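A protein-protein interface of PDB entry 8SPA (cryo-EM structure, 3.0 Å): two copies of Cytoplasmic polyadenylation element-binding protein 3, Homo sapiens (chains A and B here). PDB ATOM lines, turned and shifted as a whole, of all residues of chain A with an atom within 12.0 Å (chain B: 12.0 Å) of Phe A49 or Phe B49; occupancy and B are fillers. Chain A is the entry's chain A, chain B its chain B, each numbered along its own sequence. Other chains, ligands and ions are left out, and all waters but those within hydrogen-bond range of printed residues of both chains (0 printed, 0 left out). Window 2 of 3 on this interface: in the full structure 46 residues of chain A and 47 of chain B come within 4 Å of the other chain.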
ATOM      1  N   THR A  11       7.286  27.928  -6.970  1.00  0.00           N
ATOM      2  CA  THR A  11       8.537  27.482  -7.571  1.00  0.00           C
ATOM      3  C   THR A  11       8.352  26.990  -9.000  1.00  0.00           C
ATOM      4  O   THR A  11       9.165  27.299  -9.873  1.00  0.00           O
ATOM      5  CB  THR A  11       9.166  26.380  -6.716  1.00  0.00           C
ATOM      6  OG1 THR A  11       9.421  26.886  -5.402  1.00  0.00           O
ATOM      7  CG2 THR A  11      10.469  25.914  -7.331  1.00  0.00           C
ATOM      8  N   GLY A  12       7.298  26.226  -9.256  1.00  0.00           N
ATOM      9  CA  GLY A  12       7.016  25.741 -10.587  1.00  0.00           C
ATOM     10  C   GLY A  12       6.155  26.707 -11.375  1.00  0.00           C
ATOM     11  O   GLY A  12       5.932  27.855 -10.993  1.00  0.00           O
ATOM     12  N   THR A  13       5.654  26.212 -12.502  1.00  0.00           N
ATOM     13  CA  THR A  13       4.821  27.027 -13.373  1.00  0.00           C
ATOM     14  C   THR A  13       3.523  27.412 -12.679  1.00  0.00           C
ATOM     15  O   THR A  13       3.080  26.749 -11.739  1.00  0.00           O
ATOM     16  CB  THR A  13       4.521  26.278 -14.669  1.00  0.00           C
ATOM     17  OG1 THR A  13       3.844  27.149 -15.580  1.00  0.00           O
ATOM     18  CG2 THR A  13       3.656  25.087 -14.399  1.00  0.00           C
ATOM     19  N   PHE A  45      -6.459  18.356 -18.494  1.00  0.00           N
ATOM     20  CA  PHE A  45      -5.659  18.658 -17.316  1.00  0.00           C
ATOM     21  C   PHE A  45      -4.795  17.451 -16.985  1.00  0.00           C
ATOM     22  O   PHE A  45      -5.228  16.308 -17.161  1.00  0.00           O
ATOM     23  CB  PHE A  45      -6.536  19.014 -16.116  1.00  0.00           C
ATOM     24  CG  PHE A  45      -7.390  20.227 -16.323  1.00  0.00           C
ATOM     25  CD1 PHE A  45      -8.507  20.176 -17.131  1.00  0.00           C
ATOM     26  CD2 PHE A  45      -7.077  21.419 -15.706  1.00  0.00           C
ATOM     27  CE1 PHE A  45      -9.292  21.286 -17.318  1.00  0.00           C
ATOM     28  CE2 PHE A  45      -7.862  22.533 -15.892  1.00  0.00           C
ATOM     29  CZ  PHE A  45      -8.970  22.465 -16.701  1.00  0.00           C
ATOM     30  N   GLY A  46      -3.588  17.703 -16.491  1.00  0.00           N
ATOM     31  CA  GLY A  46      -2.631  16.639 -16.264  1.00  0.00           C
ATOM     32  C   GLY A  46      -2.538  16.200 -14.813  1.00  0.00           C
ATOM     33  O   GLY A  46      -2.755  16.979 -13.893  1.00  0.00           O
ATOM     34  N   GLY A  47      -2.206  14.929 -14.629  1.00  0.00           N
ATOM     35  CA  GLY A  47      -1.975  14.353 -13.318  1.00  0.00           C
ATOM     36  C   GLY A  47      -0.537  14.500 -12.874  1.00  0.00           C
ATOM     37  O   GLY A  47       0.216  15.329 -13.391  1.00  0.00           O
ATOM     38  N   THR A  48      -0.148  13.693 -11.890  1.00  0.00           N
ATOM     39  CA  THR A  48       1.210  13.737 -11.361  1.00  0.00           C
ATOM     40  C   THR A  48       1.716  12.317 -11.166  1.00  0.00           C
ATOM     41  O   THR A  48       0.945  11.356 -11.148  1.00  0.00           O
ATOM     42  CB  THR A  48       1.283  14.501 -10.037  1.00  0.00           C
ATOM     43  OG1 THR A  48       0.473  13.839  -9.061  1.00  0.00           O
ATOM     44  CG2 THR A  48       0.799  15.924 -10.207  1.00  0.00           C
ATOM     45  N   PHE A  49       3.033  12.198 -11.015  1.00  0.00           N
ATOM     46  CA  PHE A  49       3.661  10.929 -10.669  1.00  0.00           C
ATOM     47  C   PHE A  49       4.296  10.991  -9.286  1.00  0.00           C
ATOM     48  O   PHE A  49       5.473  10.676  -9.119  1.00  0.00           O
ATOM     49  CB  PHE A  49       4.718  10.536 -11.699  1.00  0.00           C
ATOM     50  CG  PHE A  49       4.154  10.184 -13.042  1.00  0.00           C
ATOM     51  CD1 PHE A  49       2.803   9.935 -13.199  1.00  0.00           C
ATOM     52  CD2 PHE A  49       4.981  10.071 -14.143  1.00  0.00           C
ATOM     53  CE1 PHE A  49       2.281   9.604 -14.435  1.00  0.00           C
ATOM     54  CE2 PHE A  49       4.467   9.737 -15.380  1.00  0.00           C
ATOM     55  CZ  PHE A  49       3.115   9.502 -15.526  1.00  0.00           C
ATOM     56  N   PHE B  45      -3.267  21.654 -20.729  1.00  0.00           N
ATOM     57  CA  PHE B  45      -2.518  22.005 -19.528  1.00  0.00           C
ATOM     58  C   PHE B  45      -1.631  20.833 -19.140  1.00  0.00           C
ATOM     59  O   PHE B  45      -2.022  19.674 -19.309  1.00  0.00           O
ATOM     60  CB  PHE B  45      -3.450  22.357 -18.369  1.00  0.00           C
ATOM     61  CG  PHE B  45      -4.333  23.537 -18.632  1.00  0.00           C
ATOM     62  CD1 PHE B  45      -5.418  23.435 -19.479  1.00  0.00           C
ATOM     63  CD2 PHE B  45      -4.082  24.751 -18.029  1.00  0.00           C
ATOM     64  CE1 PHE B  45      -6.230  24.515 -19.717  1.00  0.00           C
ATOM     65  CE2 PHE B  45      -4.892  25.835 -18.267  1.00  0.00           C
ATOM     66  CZ  PHE B  45      -5.968  25.716 -19.113  1.00  0.00           C
ATOM     67  N   GLY B  46      -0.451  21.133 -18.610  1.00  0.00           N
ATOM     68  CA  GLY B  46       0.529  20.105 -18.326  1.00  0.00           C
ATOM     69  C   GLY B  46       0.583  19.699 -16.864  1.00  0.00           C
ATOM     70  O   GLY B  46       0.308  20.489 -15.967  1.00  0.00           O
ATOM     71  N   GLY B  47       0.947  18.443 -16.640  1.00  0.00           N
ATOM     72  CA  GLY B  47       1.148  17.901 -15.311  1.00  0.00           C
ATOM     73  C   GLY B  47       2.563  18.102 -14.817  1.00  0.00           C
ATOM     74  O   GLY B  47       3.309  18.945 -15.326  1.00  0.00           O
ATOM     75  N   THR B  48       2.941  17.328 -13.803  1.00  0.00           N
ATOM     76  CA  THR B  48       4.277  17.426 -13.228  1.00  0.00           C
ATOM     77  C   THR B  48       4.819  16.026 -12.984  1.00  0.00           C
ATOM     78  O   THR B  48       4.078  15.043 -12.973  1.00  0.00           O
ATOM     79  CB  THR B  48       4.278  18.218 -11.918  1.00  0.00           C
ATOM     80  OG1 THR B  48       3.453  17.550 -10.957  1.00  0.00           O
ATOM     81  CG2 THR B  48       3.755  19.621 -12.135  1.00  0.00           C
ATOM     82  N   PHE B  49       6.133  15.954 -12.785  1.00  0.00           N
ATOM     83  CA  PHE B  49       6.787  14.711 -12.388  1.00  0.00           C
ATOM     84  C   PHE B  49       7.368  14.822 -10.985  1.00  0.00           C
ATOM     85  O   PHE B  49       8.548  14.549 -10.769  1.00  0.00           O
ATOM     86  CB  PHE B  49       7.892  14.332 -13.371  1.00  0.00           C
ATOM     87  CG  PHE B  49       7.390  13.935 -14.725  1.00  0.00           C
ATOM     88  CD1 PHE B  49       6.053  13.641 -14.926  1.00  0.00           C
ATOM     89  CD2 PHE B  49       8.259  13.828 -15.793  1.00  0.00           C
ATOM     90  CE1 PHE B  49       5.588  13.269 -16.173  1.00  0.00           C
ATOM     91  CE2 PHE B  49       7.802  13.452 -17.041  1.00  0.00           C
ATOM     92  CZ  PHE B  49       6.464  13.172 -17.231  1.00  0.00           C
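Gly A46 touches Phe B45, but with the chains exchanged Phe A45 does not touch Gly B46 (5.8 Å). Gly A47 touches Thr B48, but with the chains exchanged Thr A48 does not touch Gly B47 (5.4 Å). Phe A49 touches Thr B48, but with the chains exchanged Thr A48 does not touch Phe B49 (5.6 Å). Phe A49 touches its own counterpart, Phe B49. Positions printed for both chains: 45, 46, 47, 48 and 49. Of the 6 pairs that touch across the chains among the printed residues, 3 have their exchanged pair printed and touching as well.
Gly A12 touches none of the printed residues of chain B. Of the printed residues of chain B, Gly A46 touches Phe B45. Of chain B, only Gly B47 (3.3 Å) and Thr B48 (3.4 Å) come within 4 Å of Gly A47. Phe A49 touches just these residues of chain B: Thr B48 (3.6 Å) and Phe B49 (3.8 Å). Of the printed residues of chain A, Phe B45 touches Gly A46. Of the printed residues of chain A, Gly B47 touches Gly A47 (3.3 Å). Phe B49 touches one residue of chain A. The nearest residue of chain B that does not touch Phe A49 is Gly B47 (7.0 Å).
Among the printed residues, merely in contact across the chains: Gly A46 with Phe B45, Gly A47 with Gly B47, Thr A48 with Thr B48, Phe A49 with Thr B48 and Phe A49 with Phe B49.
N of Thr B48 lies within hydrogen-bond range of O of Gly A47 (3.4 Å).
Of the 8 printed residues of chain A, 4 touch a printed residue of chain B. Of the 5 printed residues of chain B, 4 touch a printed residue of chain A. Hydrophobic or aromatic side chains of chain B within 4 Å of the printed part of chain A: Phe B49. Among the printed residues, 6 pairs touch across the chains.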
